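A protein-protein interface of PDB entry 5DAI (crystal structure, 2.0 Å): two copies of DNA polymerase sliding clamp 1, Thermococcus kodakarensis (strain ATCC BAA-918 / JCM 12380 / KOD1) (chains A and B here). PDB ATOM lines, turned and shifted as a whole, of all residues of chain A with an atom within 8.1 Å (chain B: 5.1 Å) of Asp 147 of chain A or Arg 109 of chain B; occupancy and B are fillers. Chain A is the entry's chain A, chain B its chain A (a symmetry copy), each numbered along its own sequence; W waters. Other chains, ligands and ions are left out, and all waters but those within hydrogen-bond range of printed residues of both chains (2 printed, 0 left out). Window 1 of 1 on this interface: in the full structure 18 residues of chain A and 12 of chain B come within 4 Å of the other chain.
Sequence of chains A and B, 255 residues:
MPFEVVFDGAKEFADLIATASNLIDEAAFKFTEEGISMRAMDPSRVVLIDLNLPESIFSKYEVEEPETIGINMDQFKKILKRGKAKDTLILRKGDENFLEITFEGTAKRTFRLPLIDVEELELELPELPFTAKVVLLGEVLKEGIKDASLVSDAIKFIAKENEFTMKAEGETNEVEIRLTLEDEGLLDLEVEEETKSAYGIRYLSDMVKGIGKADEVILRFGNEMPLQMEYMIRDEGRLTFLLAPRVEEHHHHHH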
ATOM      1  N   GLU A 139     -23.332 -14.343  25.606  1.00  0.00           N
ATOM      2  CA  GLU A 139     -24.335 -13.467  26.222  1.00  0.00           C
ATOM      3  C   GLU A 139     -23.984 -11.976  26.102  1.00  0.00           C
ATOM      4  O   GLU A 139     -24.801 -11.164  25.637  1.00  0.00           O
ATOM      5  CB  GLU A 139     -24.512 -13.846  27.689  1.00  0.00           C
ATOM      6  CG  GLU A 139     -25.714 -13.209  28.345  1.00  0.00           C
ATOM      7  CD  GLU A 139     -25.519 -13.000  29.835  1.00  0.00           C
ATOM      8  OE1 GLU A 139     -24.560 -13.574  30.399  1.00  0.00           O
ATOM      9  OE2 GLU A 139     -26.317 -12.245  30.436  1.00  0.00           O
ATOM     10  N   VAL A 140     -22.759 -11.619  26.496  1.00  0.00           N
ATOM     11  CA  VAL A 140     -22.303 -10.225  26.443  1.00  0.00           C
ATOM     12  C   VAL A 140     -22.269  -9.689  25.017  1.00  0.00           C
ATOM     13  O   VAL A 140     -22.719  -8.574  24.751  1.00  0.00           O
ATOM     14  CB  VAL A 140     -20.895 -10.058  27.065  1.00  0.00           C
ATOM     15  CG1 VAL A 140     -20.351  -8.637  26.824  1.00  0.00           C
ATOM     16  CG2 VAL A 140     -20.940 -10.397  28.547  1.00  0.00           C
ATOM     17  N   LEU A 141     -21.734 -10.497  24.104  1.00  0.00           N
ATOM     18  CA  LEU A 141     -21.654 -10.131  22.702  1.00  0.00           C
ATOM     19  C   LEU A 141     -23.035  -9.910  22.093  1.00  0.00           C
ATOM     20  O   LEU A 141     -23.282  -8.903  21.434  1.00  0.00           O
ATOM     21  CB  LEU A 141     -20.902 -11.223  21.919  1.00  0.00           C
ATOM     22  CG  LEU A 141     -20.517 -10.929  20.471  1.00  0.00           C
ATOM     23  CD1 LEU A 141     -19.688  -9.665  20.435  1.00  0.00           C
ATOM     24  CD2 LEU A 141     -19.731 -12.098  19.871  1.00  0.00           C
ATOM     25  N   LYS A 142     -23.915 -10.890  22.278  1.00  0.00           N
ATOM     26  CA  LYS A 142     -25.268 -10.831  21.720  1.00  0.00           C
ATOM     27  C   LYS A 142     -26.052  -9.629  22.281  1.00  0.00           C
ATOM     28  O   LYS A 142     -26.645  -8.852  21.524  1.00  0.00           O
ATOM     29  CB  LYS A 142     -26.008 -12.140  22.009  1.00  0.00           C
ATOM     30  CG  LYS A 142     -25.436 -13.361  21.263  1.00  0.00           C
ATOM     31  CD  LYS A 142     -25.735 -14.680  21.990  1.00  0.00           C
ATOM     32  CE  LYS A 142     -27.230 -15.046  21.897  1.00  0.00           C
ATOM     33  NZ  LYS A 142     -27.633 -15.410  20.514  1.00  0.00           N
ATOM     34  N   GLU A 143     -26.044  -9.496  23.607  1.00  0.00           N
ATOM     35  CA  GLU A 143     -26.571  -8.308  24.314  1.00  0.00           C
ATOM     36  C   GLU A 143     -26.097  -6.983  23.728  1.00  0.00           C
ATOM     37  O   GLU A 143     -26.892  -6.119  23.337  1.00  0.00           O
ATOM     38  CB  GLU A 143     -26.119  -8.322  25.773  1.00  0.00           C
ATOM     39  CG  GLU A 143     -27.138  -8.581  26.825  1.00  0.00           C
ATOM     40  CD  GLU A 143     -26.475  -8.593  28.188  1.00  0.00           C
ATOM     41  OE1 GLU A 143     -25.244  -8.351  28.232  1.00  0.00           O
ATOM     42  OE2 GLU A 143     -27.166  -8.837  29.199  1.00  0.00           O
ATOM     43  N   GLY A 144     -24.775  -6.821  23.725  1.00  0.00           N
ATOM     44  CA  GLY A 144     -24.146  -5.564  23.356  1.00  0.00           C
ATOM     45  C   GLY A 144     -24.473  -5.147  21.945  1.00  0.00           C
ATOM     46  O   GLY A 144     -24.626  -3.959  21.662  1.00  0.00           O
ATOM     47  N   ILE A 145     -24.591  -6.130  21.053  1.00  0.00           N
ATOM     48  CA  ILE A 145     -24.929  -5.850  19.667  1.00  0.00           C
ATOM     49  C   ILE A 145     -26.370  -5.352  19.598  1.00  0.00           C
ATOM     50  O   ILE A 145     -26.678  -4.389  18.898  1.00  0.00           O
ATOM     51  CB  ILE A 145     -24.730  -7.099  18.770  1.00  0.00           C
ATOM     52  CG1 ILE A 145     -23.225  -7.405  18.647  1.00  0.00           C
ATOM     53  CG2 ILE A 145     -25.333  -6.866  17.374  1.00  0.00           C
ATOM     54  CD1 ILE A 145     -22.898  -8.740  17.979  1.00  0.00           C
ATOM     55  N   LYS A 146     -27.244  -6.002  20.355  1.00  0.00           N
ATOM     56  CA  LYS A 146     -28.634  -5.582  20.407  1.00  0.00           C
ATOM     57  C   LYS A 146     -28.698  -4.197  21.063  1.00  0.00           C
ATOM     58  O   LYS A 146     -29.408  -3.315  20.596  1.00  0.00           O
ATOM     59  CB  LYS A 146     -29.482  -6.614  21.162  1.00  0.00           C
ATOM     60  CG  LYS A 146     -30.979  -6.416  21.038  1.00  0.00           C
ATOM     61  CD  LYS A 146     -31.416  -6.349  19.578  1.00  0.00           C
ATOM     62  CE  LYS A 146     -32.625  -5.435  19.400  1.00  0.00           C
ATOM     63  NZ  LYS A 146     -32.309  -4.020  19.795  1.00  0.00           N
ATOM     64  N   ASP A 147     -27.924  -3.993  22.118  1.00  0.00           N
ATOM     65  CA  ASP A 147     -27.888  -2.667  22.767  1.00  0.00           C
ATOM     66  C   ASP A 147     -27.524  -1.578  21.776  1.00  0.00           C
ATOM     67  O   ASP A 147     -28.191  -0.543  21.703  1.00  0.00           O
ATOM     68  CB  ASP A 147     -26.890  -2.629  23.914  1.00  0.00           C
ATOM     69  CG  ASP A 147     -27.276  -3.529  25.056  1.00  0.00           C
ATOM     70  OD1 ASP A 147     -28.469  -3.886  25.183  1.00  0.00           O
ATOM     71  OD2 ASP A 147     -26.372  -3.876  25.839  1.00  0.00           O
ATOM     72  N   ALA A 148     -26.471  -1.833  20.998  1.00  0.00           N
ATOM     73  CA  ALA A 148     -25.923  -0.839  20.086  1.00  0.00           C
ATOM     74  C   ALA A 148     -26.897  -0.504  18.959  1.00  0.00           C
ATOM     75  O   ALA A 148     -26.938   0.639  18.491  1.00  0.00           O
ATOM     76  CB  ALA A 148     -24.581  -1.325  19.505  1.00  0.00           C
ATOM     77  N   SER A 149     -27.677  -1.496  18.524  1.00  0.00           N
ATOM     78  CA  SER A 149     -28.604  -1.285  17.417  1.00  0.00           C
ATOM     79  C   SER A 149     -29.735  -0.311  17.790  1.00  0.00           C
ATOM     80  O   SER A 149     -30.429   0.203  16.916  1.00  0.00           O
ATOM     81  CB  SER A 149     -29.194  -2.622  16.936  1.00  0.00           C
ATOM     82  OG  SER A 149     -30.173  -3.098  17.840  1.00  0.00           O
ATOM     83  N   LEU A 150     -29.906  -0.048  19.084  1.00  0.00           N
ATOM     84  CA  LEU A 150     -30.873   0.952  19.537  1.00  0.00           C
ATOM     85  C   LEU A 150     -30.461   2.335  19.094  1.00  0.00           C
ATOM     86  O   LEU A 150     -31.282   3.238  19.004  1.00  0.00           O
ATOM     87  CB  LEU A 150     -31.013   0.941  21.059  1.00  0.00           C
ATOM     88  CG  LEU A 150     -32.106   0.099  21.704  1.00  0.00           C
ATOM     89  CD1 LEU A 150     -31.827  -1.383  21.521  1.00  0.00           C
ATOM     90  CD2 LEU A 150     -32.210   0.447  23.163  1.00  0.00           C
ATOM     91  N   VAL A 151     -29.173   2.481  18.804  1.00  0.00           N
ATOM     92  CA  VAL A 151     -28.510   3.778  18.744  1.00  0.00           C
ATOM     93  C   VAL A 151     -27.838   4.095  17.398  1.00  0.00           C
ATOM     94  O   VAL A 151     -27.668   5.264  17.033  1.00  0.00           O
ATOM     95  CB  VAL A 151     -27.454   3.841  19.872  1.00  0.00           C
ATOM     96  CG1 VAL A 151     -26.722   5.146  19.867  1.00  0.00           C
ATOM     97  CG2 VAL A 151     -28.130   3.616  21.213  1.00  0.00           C
ATOM     98  N   SER A 152     -27.471   3.052  16.655  1.00  0.00           N
ATOM     99  CA  SER A 152     -26.641   3.229  15.477  1.00  0.00           C
ATOM    100  C   SER A 152     -26.730   2.012  14.561  1.00  0.00           C
ATOM    101  O   SER A 152     -27.302   0.981  14.935  1.00  0.00           O
ATOM    102  CB  SER A 152     -25.179   3.477  15.897  1.00  0.00           C
ATOM    103  OG  SER A 152     -24.310   3.566  14.780  1.00  0.00           O
ATOM    104  N   ILE A 155     -20.924  -0.234  15.245  1.00  0.00           N
ATOM    105  CA  ILE A 155     -20.377  -0.419  16.578  1.00  0.00           C
ATOM    106  C   ILE A 155     -18.843  -0.416  16.539  1.00  0.00           C
ATOM    107  O   ILE A 155     -18.211  -1.054  15.687  1.00  0.00           O
ATOM    108  CB  ILE A 155     -20.906  -1.715  17.201  1.00  0.00           C
ATOM    109  CG1 ILE A 155     -20.557  -1.839  18.677  1.00  0.00           C
ATOM    110  CG2 ILE A 155     -20.368  -2.926  16.470  1.00  0.00           C
ATOM    111  CD1 ILE A 155     -21.271  -3.070  19.301  1.00  0.00           C
ATOM    112  N   MET A 166     -17.311  -1.992  23.706  1.00  0.00           N
ATOM    113  CA  MET A 166     -18.042  -1.799  22.470  1.00  0.00           C
ATOM    114  C   MET A 166     -18.846  -0.549  22.653  1.00  0.00           C
ATOM    115  O   MET A 166     -19.510  -0.384  23.676  1.00  0.00           O
ATOM    116  CB  MET A 166     -18.942  -2.992  22.152  1.00  0.00           C
ATOM    117  CG  MET A 166     -18.156  -4.261  21.906  1.00  0.00           C
ATOM    118  SD  MET A 166     -19.209  -5.705  21.784  1.00  0.00           S
ATOM    119  CE  MET A 166     -19.705  -5.992  23.474  1.00  0.00           C
ATOM    120  N   ALA A 168     -21.467   2.484  20.684  1.00  0.00           N
ATOM    121  CA  ALA A 168     -22.299   2.945  19.597  1.00  0.00           C
ATOM    122  C   ALA A 168     -22.777   4.346  19.950  1.00  0.00           C
ATOM    123  O   ALA A 168     -23.065   4.626  21.105  1.00  0.00           O
ATOM    124  CB  ALA A 168     -23.474   2.006  19.388  1.00  0.00           C
ATOM    125  N   GLU A 174     -26.169   7.296  23.239  1.00  0.00           N
ATOM    126  CA  GLU A 174     -24.982   6.440  23.150  1.00  0.00           C
ATOM    127  C   GLU A 174     -25.133   5.206  24.025  1.00  0.00           C
ATOM    128  O   GLU A 174     -25.884   5.209  25.003  1.00  0.00           O
ATOM    129  CB  GLU A 174     -23.705   7.154  23.588  1.00  0.00           C
ATOM    130  CG  GLU A 174     -23.598   8.627  23.311  1.00  0.00           C
ATOM    131  CD  GLU A 174     -22.322   9.184  23.906  1.00  0.00           C
ATOM    132  OE1 GLU A 174     -21.571   8.381  24.504  1.00  0.00           O
ATOM    133  OE2 GLU A 174     -22.065  10.400  23.780  1.00  0.00           O
ATOM    134  N   VAL A 175     -24.409   4.151  23.680  1.00  0.00           N
ATOM    135  CA  VAL A 175     -24.229   3.060  24.619  1.00  0.00           C
ATOM    136  C   VAL A 175     -22.782   2.573  24.588  1.00  0.00           C
ATOM    137  O   VAL A 175     -22.093   2.651  23.573  1.00  0.00           O
ATOM    138  CB  VAL A 175     -25.209   1.882  24.360  1.00  0.00           C
ATOM    139  CG1 VAL A 175     -24.926   1.215  23.047  1.00  0.00           C
ATOM    140  CG2 VAL A 175     -25.134   0.861  25.503  1.00  0.00           C
ATOM    141  N   GLU A 176     -22.322   2.139  25.750  1.00  0.00           N
ATOM    142  CA  GLU A 176     -21.027   1.528  25.900  1.00  0.00           C
ATOM    143  C   GLU A 176     -21.244   0.253  26.676  1.00  0.00           C
ATOM    144  O   GLU A 176     -21.966   0.241  27.675  1.00  0.00           O
ATOM    145  CB  GLU A 176     -20.046   2.446  26.640  1.00  0.00           C
ATOM    146  CG  GLU A 176     -19.740   3.737  25.916  1.00  0.00           C
ATOM    147  CD  GLU A 176     -18.641   4.551  26.595  1.00  0.00           C
ATOM    148  OE1 GLU A 176     -17.900   3.990  27.435  1.00  0.00           O
ATOM    149  OE2 GLU A 176     -18.527   5.759  26.291  1.00  0.00           O
ATOM    150  N   ILE A 177     -20.627  -0.818  26.203  1.00  0.00           N
ATOM    151  CA  ILE A 177     -20.619  -2.083  26.913  1.00  0.00           C
ATOM    152  C   ILE A 177     -19.168  -2.341  27.295  1.00  0.00           C
ATOM    153  O   ILE A 177     -18.313  -2.490  26.422  1.00  0.00           O
ATOM    154  CB  ILE A 177     -21.198  -3.243  26.046  1.00  0.00           C
ATOM    155  CG1 ILE A 177     -22.625  -2.917  25.581  1.00  0.00           C
ATOM    156  CG2 ILE A 177     -21.167  -4.552  26.808  1.00  0.00           C
ATOM    157  CD1 ILE A 177     -22.698  -2.237  24.228  1.00  0.00           C
ATOM    158  N   ARG A 178     -18.883  -2.358  28.592  1.00  0.00           N
ATOM    159  CA  ARG A 178     -17.497  -2.483  29.048  1.00  0.00           C
ATOM    160  C   ARG A 178     -17.242  -3.792  29.806  1.00  0.00           C
ATOM    161  O   ARG A 178     -18.034  -4.214  30.652  1.00  0.00           O
ATOM    162  CB  ARG A 178     -17.109  -1.278  29.920  1.00  0.00           C
ATOM    163  CG  ARG A 178     -15.714  -1.374  30.545  1.00  0.00           C
ATOM    164  CD  ARG A 178     -15.083  -0.005  30.753  1.00  0.00           C
ATOM    165  NE  ARG A 178     -15.199   0.827  29.556  1.00  0.00           N
ATOM    166  CZ  ARG A 178     -14.524   1.956  29.359  1.00  0.00           C
ATOM    167  NH1 ARG A 178     -13.662   2.384  30.276  1.00  0.00           N
ATOM    168  NH2 ARG A 178     -14.700   2.653  28.242  1.00  0.00           N
ATOM    169  N   LEU A 179     -16.139  -4.449  29.467  1.00  0.00           N
ATOM    170  CA  LEU A 179     -15.664  -5.583  30.234  1.00  0.00           C
ATOM    171  C   LEU A 179     -14.263  -5.285  30.775  1.00  0.00           C
ATOM    172  O   LEU A 179     -13.446  -4.653  30.102  1.00  0.00           O
ATOM    173  CB  LEU A 179     -15.650  -6.851  29.379  1.00  0.00           C
ATOM    174  CG  LEU A 179     -16.940  -7.559  28.961  1.00  0.00           C
ATOM    175  CD1 LEU A 179     -16.630  -8.643  27.904  1.00  0.00           C
ATOM    176  CD2 LEU A 179     -17.615  -8.189  30.168  1.00  0.00           C
ATOM    177  N   ILE A 201     -23.554  -3.367  12.422  1.00  0.00           N
ATOM    178  CA  ILE A 201     -24.415  -4.093  13.340  1.00  0.00           C
ATOM    179  C   ILE A 201     -25.272  -5.148  12.636  1.00  0.00           C
ATOM    180  O   ILE A 201     -25.484  -6.228  13.175  1.00  0.00           O
ATOM    181  CB  ILE A 201     -25.309  -3.108  14.123  1.00  0.00           C
ATOM    182  CG1 ILE A 201     -24.428  -2.265  15.046  1.00  0.00           C
ATOM    183  CG2 ILE A 201     -26.365  -3.850  14.922  1.00  0.00           C
ATOM    184  CD1 ILE A 201     -25.197  -1.464  16.070  1.00  0.00           C
ATOM    185  N   LYS A 213     -25.741 -18.288  24.773  1.00  0.00           N
ATOM    186  CA  LYS A 213     -25.440 -17.320  25.842  1.00  0.00           C
ATOM    187  C   LYS A 213     -24.177 -17.668  26.638  1.00  0.00           C
ATOM    188  O   LYS A 213     -23.402 -16.789  27.035  1.00  0.00           O
ATOM    189  CB  LYS A 213     -26.622 -17.206  26.821  1.00  0.00           C
ATOM    190  CG  LYS A 213     -27.829 -16.399  26.310  1.00  0.00           C
ATOM    191  CD  LYS A 213     -27.389 -15.173  25.507  1.00  0.00           C
ATOM    192  CE  LYS A 213     -28.545 -14.212  25.206  1.00  0.00           C
ATOM    193  NZ  LYS A 213     -28.349 -12.870  25.847  1.00  0.00           N
ATOM    194  N   ARG B  82     -33.808  -3.345  27.874  1.00  0.00           N
ATOM    195  CA  ARG B  82     -32.563  -4.076  27.636  1.00  0.00           C
ATOM    196  C   ARG B  82     -32.044  -4.738  28.914  1.00  0.00           C
ATOM    197  O   ARG B  82     -31.174  -5.597  28.856  1.00  0.00           O
ATOM    198  CB  ARG B  82     -31.494  -3.156  27.034  1.00  0.00           C
ATOM    199  CG  ARG B  82     -31.852  -2.670  25.624  1.00  0.00           C
ATOM    200  CD  ARG B  82     -31.491  -3.685  24.506  1.00  0.00           C
ATOM    201  NE  ARG B  82     -32.073  -5.016  24.675  1.00  0.00           N
ATOM    202  CZ  ARG B  82     -31.380  -6.145  24.809  1.00  0.00           C
ATOM    203  NH1 ARG B  82     -30.050  -6.142  24.792  1.00  0.00           N
ATOM    204  NH2 ARG B  82     -32.029  -7.292  24.955  1.00  0.00           N
ATOM    205  N   GLY B  83     -32.603  -4.358  30.063  1.00  0.00           N
ATOM    206  CA  GLY B  83     -32.164  -4.905  31.337  1.00  0.00           C
ATOM    207  C   GLY B  83     -32.577  -6.352  31.537  1.00  0.00           C
ATOM    208  O   GLY B  83     -33.721  -6.719  31.279  1.00  0.00           O
ATOM    209  N   LYS B  84     -31.645  -7.185  31.980  1.00  0.00           N
ATOM    210  CA  LYS B  84     -31.975  -8.573  32.268  1.00  0.00           C
ATOM    211  C   LYS B  84     -32.399  -8.705  33.732  1.00  0.00           C
ATOM    212  O   LYS B  84     -32.095  -7.848  34.563  1.00  0.00           O
ATOM    213  CB  LYS B  84     -30.790  -9.496  31.961  1.00  0.00           C
ATOM    214  CG  LYS B  84     -30.205  -9.349  30.555  1.00  0.00           C
ATOM    215  CD  LYS B  84     -31.200  -9.727  29.460  1.00  0.00           C
ATOM    216  CE  LYS B  84     -30.569  -9.624  28.058  1.00  0.00           C
ATOM    217  NZ  LYS B  84     -29.473 -10.626  27.842  1.00  0.00           N
ATOM    218  N   ASP B  87     -29.704  -8.290  36.209  1.00  0.00           N
ATOM    219  CA  ASP B  87     -28.974  -7.016  36.211  1.00  0.00           C
ATOM    220  C   ASP B  87     -29.290  -6.112  37.405  1.00  0.00           C
ATOM    221  O   ASP B  87     -30.443  -6.005  37.844  1.00  0.00           O
ATOM    222  CB  ASP B  87     -29.262  -6.229  34.930  1.00  0.00           C
ATOM    223  CG  ASP B  87     -28.499  -6.754  33.731  1.00  0.00           C
ATOM    224  OD1 ASP B  87     -27.343  -7.195  33.906  1.00  0.00           O
ATOM    225  OD2 ASP B  87     -29.056  -6.690  32.607  1.00  0.00           O
ATOM    226  N   ILE B 101     -28.058   5.492  32.303  1.00  0.00           N
ATOM    227  CA  ILE B 101     -28.723   4.262  32.708  1.00  0.00           C
ATOM    228  C   ILE B 101     -27.729   3.114  32.541  1.00  0.00           C
ATOM    229  O   ILE B 101     -27.272   2.841  31.436  1.00  0.00           O
ATOM    230  CB  ILE B 101     -30.000   4.002  31.876  1.00  0.00           C
ATOM    231  CG1 ILE B 101     -30.910   5.233  31.892  1.00  0.00           C
ATOM    232  CG2 ILE B 101     -30.762   2.785  32.398  1.00  0.00           C
ATOM    233  CD1 ILE B 101     -31.780   5.346  30.678  1.00  0.00           C
ATOM    234  N   THR B 102     -27.391   2.446  33.638  1.00  0.00           N
ATOM    235  CA  THR B 102     -26.412   1.374  33.578  1.00  0.00           C
ATOM    236  C   THR B 102     -26.991   0.057  34.104  1.00  0.00           C
ATOM    237  O   THR B 102     -27.706   0.018  35.104  1.00  0.00           O
ATOM    238  CB  THR B 102     -25.132   1.759  34.359  1.00  0.00           C
ATOM    239  OG1 THR B 102     -24.499   2.847  33.684  1.00  0.00           O
ATOM    240  CG2 THR B 102     -24.158   0.599  34.438  1.00  0.00           C
ATOM    241  N   PHE B 103     -26.711  -1.015  33.377  1.00  0.00           N
ATOM    242  CA  PHE B 103     -27.050  -2.358  33.816  1.00  0.00           C
ATOM    243  C   PHE B 103     -25.763  -3.058  34.203  1.00  0.00           C
ATOM    244  O   PHE B 103     -24.867  -3.206  33.366  1.00  0.00           O
ATOM    245  CB  PHE B 103     -27.783  -3.139  32.713  1.00  0.00           C
ATOM    246  CG  PHE B 103     -28.998  -2.431  32.172  1.00  0.00           C
ATOM    247  CD1 PHE B 103     -30.158  -2.355  32.928  1.00  0.00           C
ATOM    248  CD2 PHE B 103     -28.975  -1.845  30.913  1.00  0.00           C
ATOM    249  CE1 PHE B 103     -31.282  -1.701  32.441  1.00  0.00           C
ATOM    250  CE2 PHE B 103     -30.090  -1.187  30.420  1.00  0.00           C
ATOM    251  CZ  PHE B 103     -31.250  -1.112  31.192  1.00  0.00           C
ATOM    252  N   ALA B 107     -21.632  -7.951  32.293  1.00  0.00           N
ATOM    253  CA  ALA B 107     -20.908  -6.800  31.757  1.00  0.00           C
ATOM    254  C   ALA B 107     -21.515  -5.496  32.297  1.00  0.00           C
ATOM    255  O   ALA B 107     -22.597  -5.510  32.892  1.00  0.00           O
ATOM    256  CB  ALA B 107     -20.940  -6.816  30.239  1.00  0.00           C
ATOM    257  N   LYS B 108     -20.820  -4.378  32.092  1.00  0.00           N
ATOM    258  CA  LYS B 108     -21.339  -3.053  32.451  1.00  0.00           C
ATOM    259  C   LYS B 108     -21.829  -2.387  31.170  1.00  0.00           C
ATOM    260  O   LYS B 108     -21.056  -2.154  30.244  1.00  0.00           O
ATOM    261  CB  LYS B 108     -20.263  -2.193  33.139  1.00  0.00           C
ATOM    262  CG  LYS B 108     -20.747  -0.870  33.748  1.00  0.00           C
ATOM    263  CD  LYS B 108     -19.549  -0.010  34.202  1.00  0.00           C
ATOM    264  CE  LYS B 108     -19.987   1.191  35.033  1.00  0.00           C
ATOM    265  NZ  LYS B 108     -18.878   1.760  35.863  1.00  0.00           N
ATOM    266  N   ARG B 109     -23.124  -2.110  31.112  1.00  0.00           N
ATOM    267  CA  ARG B 109     -23.743  -1.594  29.901  1.00  0.00           C
ATOM    268  C   ARG B 109     -24.380  -0.240  30.172  1.00  0.00           C
ATOM    269  O   ARG B 109     -25.399  -0.156  30.845  1.00  0.00           O
ATOM    270  CB  ARG B 109     -24.794  -2.579  29.378  1.00  0.00           C
ATOM    271  CG  ARG B 109     -24.251  -3.960  29.043  1.00  0.00           C
ATOM    272  CD  ARG B 109     -25.351  -4.834  28.485  1.00  0.00           C
ATOM    273  NE  ARG B 109     -26.332  -5.213  29.495  1.00  0.00           N
ATOM    274  CZ  ARG B 109     -27.627  -5.410  29.254  1.00  0.00           C
ATOM    275  NH1 ARG B 109     -28.126  -5.245  28.030  1.00  0.00           N
ATOM    276  NH2 ARG B 109     -28.430  -5.765  30.241  1.00  0.00           N
ATOM    277  N   THR B 110     -23.792   0.818  29.633  1.00  0.00           N
ATOM    278  CA  THR B 110     -24.247   2.160  29.960  1.00  0.00           C
ATOM    279  C   THR B 110     -24.861   2.863  28.764  1.00  0.00           C
ATOM    280  O   THR B 110     -24.235   2.989  27.728  1.00  0.00           O
ATOM    281  CB  THR B 110     -23.093   2.999  30.520  1.00  0.00           C
ATOM    282  OG1 THR B 110     -22.594   2.361  31.704  1.00  0.00           O
ATOM    283  CG2 THR B 110     -23.567   4.435  30.849  1.00  0.00           C
ATOM    284  N   PHE B 111     -26.103   3.304  28.926  1.00  0.00           N
ATOM    285  CA  PHE B 111     -26.796   4.107  27.929  1.00  0.00           C
ATOM    286  C   PHE B 111     -26.856   5.562  28.380  1.00  0.00           C
ATOM    287  O   PHE B 111     -26.971   5.844  29.569  1.00  0.00           O
ATOM    288  CB  PHE B 111     -28.227   3.606  27.701  1.00  0.00           C
ATOM    289  CG  PHE B 111     -28.320   2.178  27.226  1.00  0.00           C
ATOM    290  CD1 PHE B 111     -28.111   1.126  28.105  1.00  0.00           C
ATOM    291  CD2 PHE B 111     -28.665   1.894  25.917  1.00  0.00           C
ATOM    292  CE1 PHE B 111     -28.233  -0.183  27.684  1.00  0.00           C
ATOM    293  CE2 PHE B 111     -28.782   0.579  25.481  1.00  0.00           C
ATOM    294  CZ  PHE B 111     -28.569  -0.457  26.370  1.00  0.00           C
HETATM  295  O   HOH W   1     -20.200   0.712  30.424  1.00  0.00           O
HETATM  296  O   HOH W   2     -24.262  -8.293  30.923  1.00  0.00           O
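Water W2 bridges OE1 of Glu 143 of chain A and N of Ala 107 of chain B.
Water W1 lies within hydrogen-bond range of O of Lys 108 of chain B (3.0 Å), OG1 of Thr 110 of chain B (3.2 Å) and O of Glu 176 of chain A (3.3 Å).
No position is printed for both chains.
Of the 22 pairs that touch across the chains among the printed residues, none has its exchanged pair printed and touching as well.
NH1 of Arg 82 of chain B sits at hydrogen-bond distance from O of Glu 143 of chain A (3.5 Å).
The side-chain amino group (NZ) of Lys 84 of chain B is in salt-bridge range of the side-chain carboxylate (OE2) of Glu 143 of chain A (3.2 Å).
OE2 of Glu 143 of chain A is in salt-bridge range of NH2 of Arg 109 of chain B (3.5 Å).
NH1 of Arg 82 of chain B lies within salt-bridge range of OD1 of Asp 147 of chain A.
NH1 of Arg 109 of chain B is in salt-bridge range of OD2 of Asp 147 of chain A (3.1 Å).
O of Glu 176 of chain A lies within hydrogen-bond range of N of Thr 110 of chain B (2.7 Å).
The backbone NH of Arg 178 of chain A sits at hydrogen-bond distance from the backbone carbonyl oxygen of Lys 108 of chain B.
The side-chain amino group (NZ) of Lys 84 of chain B lies close to the side-chain amino group (NZ) of Lys 213 of chain A (3.2 Å).
Printed residues of chain B within 4 Å of Lys 213 of chain A: Lys 84.
Of the printed residues of chain A, Thr 110 of chain B touches Glu 174, Val 175 and Glu 176.
Ala 148 of chain A touches none of the printed residues of chain B.
The nearest residue of chain A that does not touch Arg 109 of chain B is Val 175 of chain A (4.9 Å).
N of Glu 139 of chain A is in hydrogen-bond range of O of Lys 213 of chain A, at 2.8 Å.
The backbone carbonyl oxygen of Met 166 of chain A lies within hydrogen-bond range of the backbone NH of Ile 177 of chain A (2.8 Å).
The backbone carbonyl oxygen of Ile 101 of chain B is in hydrogen-bond range of the backbone NH of Phe 111 of chain B (2.8 Å).
CG1 of Val 140 of chain A touches CB of Ala 107 of chain B, at 3.9 Å.
Lys 146 of chain A touches Arg 82 of chain B.
Leu 150 of chain A touches Arg 82 of chain B (CD1 to CD, 3.8 Å).
O of Glu 174 of chain A touches O of Thr 110 of chain B, at 3.9 Å.
Lys 108 of chain B touches Glu 176 of chain A (O to O, 3.6 Å).
Arg 178 of chain A touches Ala 107 of chain B (O to CB, 3.9 Å).
CD2 of Leu 179 of chain A touches CB of Ala 107 of chain B (3.6 Å).
Printed residues of chain B that touch a printed residue of chain A: Arg 82, Lys 84, Ala 107, Lys 108, Arg 109, Thr 110 and Phe 111.
Hydrophobic or aromatic side chains of chain B within 4 Å of the printed part of chain A: Ala 107 and Phe 111.
Along chain B the printed residues that touch a printed residue of chain A span positions 82 to 111.
Of the 25 printed residues of chain A, 12 touch a printed residue of chain B.
Printed residues of chain A that touch a printed residue of chain B: Val 140, Glu 143, Lys 146, Asp 147, Leu 150, Glu 174, Val 175, Glu 176, Ile 177, Arg 178, Leu 179 and Lys 213.
Among the printed residues, Asp or Glu carboxylates within 4 Å of a Lys or Arg side-chain nitrogen of the other chain: Glu 143 of chain A with Lys 84 of chain B (3.2 Å), Glu 143 of chain A with Arg 109 of chain B (3.5 Å), Asp 147 of chain A with Arg 82 of chain B (2.8 Å) and Asp 147 of chain A with Arg 109 of chain B (3.1 Å).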
